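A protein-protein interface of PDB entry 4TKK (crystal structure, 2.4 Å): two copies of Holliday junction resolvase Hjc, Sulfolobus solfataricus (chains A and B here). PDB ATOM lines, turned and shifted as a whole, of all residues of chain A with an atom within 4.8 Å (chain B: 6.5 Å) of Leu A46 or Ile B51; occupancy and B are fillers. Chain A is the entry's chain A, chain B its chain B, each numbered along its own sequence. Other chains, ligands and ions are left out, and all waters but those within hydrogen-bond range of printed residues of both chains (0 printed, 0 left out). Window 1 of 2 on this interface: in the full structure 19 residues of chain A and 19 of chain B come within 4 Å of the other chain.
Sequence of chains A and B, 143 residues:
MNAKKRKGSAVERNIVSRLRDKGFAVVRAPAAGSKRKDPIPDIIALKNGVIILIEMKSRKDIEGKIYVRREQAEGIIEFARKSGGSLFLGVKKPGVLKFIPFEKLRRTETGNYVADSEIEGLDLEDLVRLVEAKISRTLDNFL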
ATOM      1  N   GLY A  23       0.956  -5.101  13.005  1.00  0.00           N
ATOM      2  CA  GLY A  23       1.812  -6.176  13.480  1.00  0.00           C
ATOM      3  C   GLY A  23       3.240  -6.179  12.945  1.00  0.00           C
ATOM      4  O   GLY A  23       3.914  -7.207  13.022  1.00  0.00           O
ATOM      5  N   PHE A  24       3.720  -5.048  12.383  1.00  0.00           N
ATOM      6  CA  PHE A  24       5.092  -4.998  11.878  1.00  0.00           C
ATOM      7  C   PHE A  24       6.049  -4.593  12.963  1.00  0.00           C
ATOM      8  O   PHE A  24       5.696  -3.752  13.796  1.00  0.00           O
ATOM      9  CB  PHE A  24       5.240  -3.995  10.716  1.00  0.00           C
ATOM     10  CG  PHE A  24       4.661  -4.435   9.402  1.00  0.00           C
ATOM     11  CD1 PHE A  24       3.286  -4.399   9.180  1.00  0.00           C
ATOM     12  CD2 PHE A  24       5.488  -4.850   8.367  1.00  0.00           C
ATOM     13  CE1 PHE A  24       2.748  -4.780   7.953  1.00  0.00           C
ATOM     14  CE2 PHE A  24       4.949  -5.269   7.154  1.00  0.00           C
ATOM     15  CZ  PHE A  24       3.584  -5.204   6.944  1.00  0.00           C
ATOM     16  N   ALA A  25       7.283  -5.145  12.933  1.00  0.00           N
ATOM     17  CA  ALA A  25       8.381  -4.689  13.800  1.00  0.00           C
ATOM     18  C   ALA A  25       8.993  -3.596  12.914  1.00  0.00           C
ATOM     19  O   ALA A  25       9.363  -3.859  11.766  1.00  0.00           O
ATOM     20  CB  ALA A  25       9.387  -5.804  14.038  1.00  0.00           C
ATOM     21  N   ILE A  44      12.144   0.723   7.901  1.00  0.00           N
ATOM     22  CA  ILE A  44      12.327  -0.705   7.741  1.00  0.00           C
ATOM     23  C   ILE A  44      11.231  -1.346   8.587  1.00  0.00           C
ATOM     24  O   ILE A  44      11.175  -1.134   9.793  1.00  0.00           O
ATOM     25  CB  ILE A  44      13.745  -1.163   8.140  1.00  0.00           C
ATOM     26  CG1 ILE A  44      14.789  -0.480   7.242  1.00  0.00           C
ATOM     27  CG2 ILE A  44      13.868  -2.688   8.086  1.00  0.00           C
ATOM     28  CD1 ILE A  44      16.036  -0.251   7.873  1.00  0.00           C
ATOM     29  N   ALA A  45      10.351  -2.080   7.932  1.00  0.00           N
ATOM     30  CA  ALA A  45       9.219  -2.742   8.549  1.00  0.00           C
ATOM     31  C   ALA A  45       9.337  -4.226   8.264  1.00  0.00           C
ATOM     32  O   ALA A  45       9.583  -4.636   7.128  1.00  0.00           O
ATOM     33  CB  ALA A  45       7.921  -2.179   7.989  1.00  0.00           C
ATOM     34  N   LEU A  46       9.267  -5.015   9.322  1.00  0.00           N
ATOM     35  CA  LEU A  46       9.444  -6.447   9.254  1.00  0.00           C
ATOM     36  C   LEU A  46       8.238  -7.147   9.815  1.00  0.00           C
ATOM     37  O   LEU A  46       7.771  -6.827  10.903  1.00  0.00           O
ATOM     38  CB  LEU A  46      10.704  -6.852  10.054  1.00  0.00           C
ATOM     39  CG  LEU A  46      11.980  -6.018   9.847  1.00  0.00           C
ATOM     40  CD1 LEU A  46      12.975  -6.311  10.928  1.00  0.00           C
ATOM     41  CD2 LEU A  46      12.584  -6.246   8.458  1.00  0.00           C
ATOM     42  N   LYS A  47       7.734  -8.098   9.080  1.00  0.00           N
ATOM     43  CA  LYS A  47       6.604  -8.891   9.541  1.00  0.00           C
ATOM     44  C   LYS A  47       6.737 -10.297   9.041  1.00  0.00           C
ATOM     45  O   LYS A  47       6.723 -10.524   7.830  1.00  0.00           O
ATOM     46  CB  LYS A  47       5.248  -8.312   9.134  1.00  0.00           C
ATOM     47  CG  LYS A  47       4.133  -9.018   9.853  1.00  0.00           C
ATOM     48  CD  LYS A  47       2.780  -8.450   9.586  1.00  0.00           C
ATOM     49  CE  LYS A  47       1.748  -9.311  10.265  1.00  0.00           C
ATOM     50  NZ  LYS A  47       0.430  -8.639  10.211  1.00  0.00           N
ATOM     51  N   ASN A  48       6.931 -11.227   9.974  1.00  0.00           N
ATOM     52  CA  ASN A  48       7.014 -12.657   9.682  1.00  0.00           C
ATOM     53  C   ASN A  48       7.896 -13.026   8.495  1.00  0.00           C
ATOM     54  O   ASN A  48       7.496 -13.792   7.642  1.00  0.00           O
ATOM     55  CB  ASN A  48       5.576 -13.239   9.595  1.00  0.00           C
ATOM     56  CG  ASN A  48       4.820 -12.999  10.904  1.00  0.00           C
ATOM     57  OD1 ASN A  48       5.318 -13.243  12.028  1.00  0.00           O
ATOM     58  ND2 ASN A  48       3.639 -12.415  10.787  1.00  0.00           N
ATOM     59  N   GLY A  49       9.105 -12.480   8.464  1.00  0.00           N
ATOM     60  CA  GLY A  49      10.066 -12.775   7.414  1.00  0.00           C
ATOM     61  C   GLY A  49       9.990 -11.888   6.192  1.00  0.00           C
ATOM     62  O   GLY A  49      10.861 -11.963   5.327  1.00  0.00           O
ATOM     63  N   VAL A  50       8.957 -11.048   6.106  1.00  0.00           N
ATOM     64  CA  VAL A  50       8.808 -10.109   5.001  1.00  0.00           C
ATOM     65  C   VAL A  50       9.425  -8.786   5.424  1.00  0.00           C
ATOM     66  O   VAL A  50       9.164  -8.293   6.515  1.00  0.00           O
ATOM     67  CB  VAL A  50       7.345  -9.958   4.520  1.00  0.00           C
ATOM     68  CG1 VAL A  50       7.246  -8.951   3.383  1.00  0.00           C
ATOM     69  CG2 VAL A  50       6.796 -11.304   4.073  1.00  0.00           C
ATOM     70  N   ILE A  51      10.292  -8.256   4.565  1.00  0.00           N
ATOM     71  CA  ILE A  51      11.050  -7.044   4.769  1.00  0.00           C
ATOM     72  C   ILE A  51      10.529  -5.998   3.807  1.00  0.00           C
ATOM     73  O   ILE A  51      10.550  -6.192   2.586  1.00  0.00           O
ATOM     74  CB  ILE A  51      12.559  -7.314   4.566  1.00  0.00           C
ATOM     75  CG1 ILE A  51      13.071  -8.470   5.460  1.00  0.00           C
ATOM     76  CG2 ILE A  51      13.378  -6.028   4.769  1.00  0.00           C
ATOM     77  CD1 ILE A  51      14.403  -9.117   4.961  1.00  0.00           C
ATOM     78  N   ILE B  44      20.092  -4.741  13.723  1.00  0.00           N
ATOM     79  CA  ILE B  44      19.212  -5.463  12.815  1.00  0.00           C
ATOM     80  C   ILE B  44      20.012  -5.660  11.540  1.00  0.00           C
ATOM     81  O   ILE B  44      20.430  -4.688  10.915  1.00  0.00           O
ATOM     82  CB  ILE B  44      17.878  -4.733  12.582  1.00  0.00           C
ATOM     83  CG1 ILE B  44      17.116  -4.587  13.918  1.00  0.00           C
ATOM     84  CG2 ILE B  44      17.033  -5.446  11.500  1.00  0.00           C
ATOM     85  CD1 ILE B  44      16.299  -3.421  13.990  1.00  0.00           C
ATOM     86  N   ALA B  45      20.254  -6.909  11.190  1.00  0.00           N
ATOM     87  CA  ALA B  45      21.039  -7.315  10.044  1.00  0.00           C
ATOM     88  C   ALA B  45      20.175  -8.201   9.177  1.00  0.00           C
ATOM     89  O   ALA B  45      19.530  -9.125   9.669  1.00  0.00           O
ATOM     90  CB  ALA B  45      22.290  -8.063  10.503  1.00  0.00           C
ATOM     91  N   LEU B  46      20.091  -7.845   7.899  1.00  0.00           N
ATOM     92  CA  LEU B  46      19.239  -8.505   6.959  1.00  0.00           C
ATOM     93  C   LEU B  46      20.054  -8.992   5.799  1.00  0.00           C
ATOM     94  O   LEU B  46      20.857  -8.253   5.238  1.00  0.00           O
ATOM     95  CB  LEU B  46      18.144  -7.527   6.459  1.00  0.00           C
ATOM     96  CG  LEU B  46      17.419  -6.668   7.504  1.00  0.00           C
ATOM     97  CD1 LEU B  46      16.684  -5.537   6.861  1.00  0.00           C
ATOM     98  CD2 LEU B  46      16.490  -7.515   8.368  1.00  0.00           C
ATOM     99  N   LYS B  47      19.851 -10.231   5.431  1.00  0.00           N
ATOM    100  CA  LYS B  47      20.528 -10.783   4.282  1.00  0.00           C
ATOM    101  C   LYS B  47      19.632 -11.773   3.607  1.00  0.00           C
ATOM    102  O   LYS B  47      19.297 -12.807   4.188  1.00  0.00           O
ATOM    103  CB  LYS B  47      21.895 -11.421   4.624  1.00  0.00           C
ATOM    104  CG  LYS B  47      22.662 -11.733   3.360  1.00  0.00           C
ATOM    105  CD  LYS B  47      24.029 -12.293   3.599  1.00  0.00           C
ATOM    106  CE  LYS B  47      24.629 -12.658   2.264  1.00  0.00           C
ATOM    107  NZ  LYS B  47      26.066 -12.958   2.413  1.00  0.00           N
ATOM    108  N   GLY B  49      16.449 -12.178   2.983  1.00  0.00           N
ATOM    109  CA  GLY B  49      15.265 -12.701   3.657  1.00  0.00           C
ATOM    110  C   GLY B  49      15.490 -13.173   5.073  1.00  0.00           C
ATOM    111  O   GLY B  49      14.523 -13.411   5.795  1.00  0.00           O
ATOM    112  N   VAL B  50      16.763 -13.323   5.480  1.00  0.00           N
ATOM    113  CA  VAL B  50      17.118 -13.744   6.827  1.00  0.00           C
ATOM    114  C   VAL B  50      17.285 -12.485   7.677  1.00  0.00           C
ATOM    115  O   VAL B  50      17.974 -11.544   7.276  1.00  0.00           O
ATOM    116  CB  VAL B  50      18.336 -14.702   6.869  1.00  0.00           C
ATOM    117  CG1 VAL B  50      18.642 -15.120   8.311  1.00  0.00           C
ATOM    118  CG2 VAL B  50      18.095 -15.932   5.997  1.00  0.00           C
ATOM    119  N   ILE B  51      16.587 -12.459   8.815  1.00  0.00           N
ATOM    120  CA  ILE B  51      16.576 -11.333   9.742  1.00  0.00           C
ATOM    121  C   ILE B  51      17.292 -11.765  10.993  1.00  0.00           C
ATOM    122  O   ILE B  51      16.879 -12.723  11.634  1.00  0.00           O
ATOM    123  CB  ILE B  51      15.112 -10.870  10.050  1.00  0.00           C
ATOM    124  CG1 ILE B  51      14.326 -10.564   8.753  1.00  0.00           C
ATOM    125  CG2 ILE B  51      15.082  -9.705  11.074  1.00  0.00           C
ATOM    126  CD1 ILE B  51      12.791 -10.508   8.934  1.00  0.00           C
ATOM    127  N   ILE B  52      18.372 -11.072  11.328  1.00  0.00           N
ATOM    128  CA  ILE B  52      19.152 -11.347  12.527  1.00  0.00           C
ATOM    129  C   ILE B  52      19.039 -10.137  13.386  1.00  0.00           C
ATOM    130  O   ILE B  52      19.094  -8.989  12.902  1.00  0.00           O
ATOM    131  CB  ILE B  52      20.625 -11.766  12.232  1.00  0.00           C
ATOM    132  CG1 ILE B  52      20.799 -13.004  11.377  1.00  0.00           C
ATOM    133  CG2 ILE B  52      21.624 -11.662  13.375  1.00  0.00           C
ATOM    134  CD1 ILE B  52      19.981 -14.161  11.805  1.00  0.00           C
ATOM    135  N   LEU B  53      18.792 -10.387  14.655  1.00  0.00           N
ATOM    136  CA  LEU B  53      18.617  -9.328  15.621  1.00  0.00           C
ATOM    137  C   LEU B  53      19.587  -9.583  16.707  1.00  0.00           C
ATOM    138  O   LEU B  53      19.668 -10.694  17.226  1.00  0.00           O
ATOM    139  CB  LEU B  53      17.162  -9.282  16.161  1.00  0.00           C
ATOM    140  CG  LEU B  53      16.088  -9.277  15.087  1.00  0.00           C
ATOM    141  CD1 LEU B  53      14.731  -9.612  15.684  1.00  0.00           C
ATOM    142  CD2 LEU B  53      16.064  -7.960  14.309  1.00  0.00           C
ATOM    143  N   PHE B  79       9.715  -8.026  19.347  1.00  0.00           N
ATOM    144  CA  PHE B  79      10.239  -7.505  18.074  1.00  0.00           C
ATOM    145  C   PHE B  79      10.659  -8.703  17.183  1.00  0.00           C
ATOM    146  O   PHE B  79      10.335  -8.733  15.995  1.00  0.00           O
ATOM    147  CB  PHE B  79      11.426  -6.553  18.316  1.00  0.00           C
ATOM    148  CG  PHE B  79      11.838  -5.780  17.076  1.00  0.00           C
ATOM    149  CD1 PHE B  79      12.624  -6.375  16.089  1.00  0.00           C
ATOM    150  CD2 PHE B  79      11.459  -4.456  16.903  1.00  0.00           C
ATOM    151  CE1 PHE B  79      12.995  -5.663  14.941  1.00  0.00           C
ATOM    152  CE2 PHE B  79      11.840  -3.749  15.761  1.00  0.00           C
ATOM    153  CZ  PHE B  79      12.618  -4.352  14.794  1.00  0.00           C
ATOM    154  N   LYS B  82       7.327 -10.729  16.023  1.00  0.00           N
ATOM    155  CA  LYS B  82       6.695  -9.911  14.972  1.00  0.00           C
ATOM    156  C   LYS B  82       7.470  -9.942  13.665  1.00  0.00           C
ATOM    157  O   LYS B  82       6.866 -10.179  12.620  1.00  0.00           O
ATOM    158  CB  LYS B  82       6.608  -8.438  15.430  1.00  0.00           C
ATOM    159  CG  LYS B  82       5.386  -8.103  16.266  1.00  0.00           C
ATOM    160  CD  LYS B  82       5.127  -6.599  16.267  1.00  0.00           C
ATOM    161  CE  LYS B  82       5.523  -5.922  17.556  1.00  0.00           C
ATOM    162  NZ  LYS B  82       4.478  -6.053  18.614  1.00  0.00           N
ATOM    163  N   SER B  83       8.806  -9.667  13.715  1.00  0.00           N
ATOM    164  CA  SER B  83       9.659  -9.583  12.525  1.00  0.00           C
ATOM    165  C   SER B  83       9.913 -10.903  11.853  1.00  0.00           C
ATOM    166  O   SER B  83      10.171 -10.936  10.647  1.00  0.00           O
ATOM    167  CB  SER B  83      10.993  -8.936  12.874  1.00  0.00           C
ATOM    168  OG  SER B  83      11.766  -9.722  13.764  1.00  0.00           O
ATOM    169  N   GLY B  84       9.879 -11.976  12.639  1.00  0.00           N
ATOM    170  CA  GLY B  84      10.209 -13.317  12.169  1.00  0.00           C
ATOM    171  C   GLY B  84      11.716 -13.489  12.198  1.00  0.00           C
ATOM    172  O   GLY B  84      12.250 -14.369  11.550  1.00  0.00           O
ATOM    173  N   GLY B  85      12.416 -12.613  12.909  1.00  0.00           N
ATOM    174  CA  GLY B  85      13.870 -12.675  12.968  1.00  0.00           C
ATOM    175  C   GLY B  85      14.424 -13.468  14.132  1.00  0.00           C
ATOM    176  O   GLY B  85      13.718 -13.718  15.114  1.00  0.00           O
ATOM    177  N   SER B  86      15.697 -13.869  14.018  1.00  0.00           N
ATOM    178  CA  SER B  86      16.379 -14.639  15.052  1.00  0.00           C
ATOM    179  C   SER B  86      17.119 -13.678  15.948  1.00  0.00           C
ATOM    180  O   SER B  86      17.894 -12.861  15.482  1.00  0.00           O
ATOM    181  CB  SER B  86      17.333 -15.633  14.413  1.00  0.00           C
ATOM    182  OG  SER B  86      16.587 -16.551  13.626  1.00  0.00           O
ATOM    183  N   LEU B  87      16.804 -13.719  17.235  1.00  0.00           N
ATOM    184  CA  LEU B  87      17.371 -12.843  18.234  1.00  0.00           C
ATOM    185  C   LEU B  87      18.570 -13.478  18.939  1.00  0.00           C
ATOM    186  O   LEU B  87      18.567 -14.679  19.254  1.00  0.00           O
ATOM    187  CB  LEU B  87      16.279 -12.411  19.200  1.00  0.00           C
ATOM    188  CG  LEU B  87      16.643 -11.486  20.364  1.00  0.00           C
ATOM    189  CD1 LEU B  87      17.119 -10.107  19.886  1.00  0.00           C
ATOM    190  CD2 LEU B  87      15.454 -11.358  21.321  1.00  0.00           C
ATOM    191  N   PHE B  88      19.607 -12.662  19.151  1.00  0.00           N
ATOM    192  CA  PHE B  88      20.820 -13.083  19.826  1.00  0.00           C
ATOM    193  C   PHE B  88      21.190 -12.088  20.830  1.00  0.00           C
ATOM    194  O   PHE B  88      20.993 -10.903  20.629  1.00  0.00           O
ATOM    195  CB  PHE B  88      22.010 -13.252  18.836  1.00  0.00           C
ATOM    196  CG  PHE B  88      21.747 -14.302  17.794  1.00  0.00           C
ATOM    197  CD1 PHE B  88      21.073 -13.988  16.628  1.00  0.00           C
ATOM    198  CD2 PHE B  88      22.139 -15.614  17.996  1.00  0.00           C
ATOM    199  CE1 PHE B  88      20.768 -14.973  15.700  1.00  0.00           C
ATOM    200  CE2 PHE B  88      21.832 -16.605  17.064  1.00  0.00           C
ATOM    201  CZ  PHE B  88      21.135 -16.284  15.936  1.00  0.00           C
ATOM    202  N   VAL B 131      23.187 -18.157   8.767  1.00  0.00           N
ATOM    203  CA  VAL B 131      22.428 -17.305   7.847  1.00  0.00           C
ATOM    204  C   VAL B 131      22.552 -17.864   6.430  1.00  0.00           C
ATOM    205  O   VAL B 131      21.526 -18.092   5.783  1.00  0.00           O
ATOM    206  CB  VAL B 131      22.850 -15.814   7.946  1.00  0.00           C
ATOM    207  CG1 VAL B 131      22.187 -14.970   6.858  1.00  0.00           C
ATOM    208  CG2 VAL B 131      22.542 -15.257   9.320  1.00  0.00           C
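The backbone NH (N) of Asn A48 lies within hydrogen-bond range of the backbone carbonyl oxygen (O) of Lys B82 (2.8 Å). O of Ser B83 is in hydrogen-bond range of N of Asn A48. The backbone NH (N) of Gly A49 lies within hydrogen-bond range of the backbone carbonyl oxygen (O) of Ser B83 (2.9 Å).
Leu A46 touches Ile B51, and with the chains exchanged Ile A51 touches Leu B46. Gly A49 touches its own counterpart, Gly B49. Gly A49 touches Ile B51, and with the chains exchanged Ile A51 touches Gly B49. Positions printed for both chains: 44, 45, 46, 47, 49, 50 and 51. Of the 17 pairs that touch across the chains among the printed residues, 5 have their exchanged pair printed and touching as well.
The backbone carbonyl oxygen of Leu A46 lies within hydrogen-bond range of the backbone NH of Ala A25 (2.7 Å). The backbone carbonyl oxygen (O) of Ile B51 is in hydrogen-bond range of the backbone NH (N) of Ser B86 (2.9 Å). The backbone carbonyl oxygen (O) of Phe B79 is in hydrogen-bond range of the side-chain hydroxyl (OG) of Ser B83. N of Gly B85 is in hydrogen-bond range of OG of Ser B83 (3.1 Å).
Of the 11 printed residues of chain A, 8 touch a printed residue of chain B. Hydrophobic or aromatic side chains of chain A within 4 Å of the printed part of chain B: Ala A25, Leu A46 and Ile A51. Along chain A the printed residues that touch a printed residue of chain B span positions 23 to 51. Of the 18 printed residues of chain B, 7 touch a printed residue of chain A. Among the printed residues, 17 pairs touch across the chains. Among the printed residues, no Asp or Glu carboxylate lies within 4 Å of a Lys or Arg side-chain nitrogen of the other chain.
Among the printed residues, merely in contact across the chains: Gly A23 with Lys B82 (3.5 Å), Phe A24 with Lys B82 (3.8 Å), Ala A25 with Phe B79 (3.6 Å), Ala A25 with Ser B83 (3.7 Å), Leu A46 with Ile B51 (3.997 Å), Leu A46 with Lys B82 (3.9 Å), Leu A46 with Ser B83 (3.5 Å), Lys A47 with Lys B82 (3.3 Å), Lys A47 with Ser B83 (3.8 Å), Gly A49 with Gly B49 (3.97 Å), Gly A49 with Ile B51 (3.9 Å), Gly A49 with Gly B84 (3.96 Å), Ile A51 with Leu B46 (3.9 Å) and Ile A51 with Gly B49 (3.9 Å).
Of the printed residues of chain B, Leu A46 touches Ile B51, Lys B82 and Ser B83. Of the printed residues of chain B, Asn A48 touches Lys B82 (2.8 Å) and Ser B83 (3.3 Å). Of the printed residues of chain A, Ile B51 touches Leu A46 (3.997 Å) and Gly A49 (3.9 Å). Printed residues of chain A within 4 Å of Gly B84: Gly A49. The nearest printed residue of chain B that does not touch Leu A46 is Phe B79 (4.1 Å). The nearest printed residue of chain A that does not touch Ile B51 is Ile A51 (4.04 Å). The nearest printed residue of chain A that does not touch Phe B79 is Leu A46 (4.1 Å).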
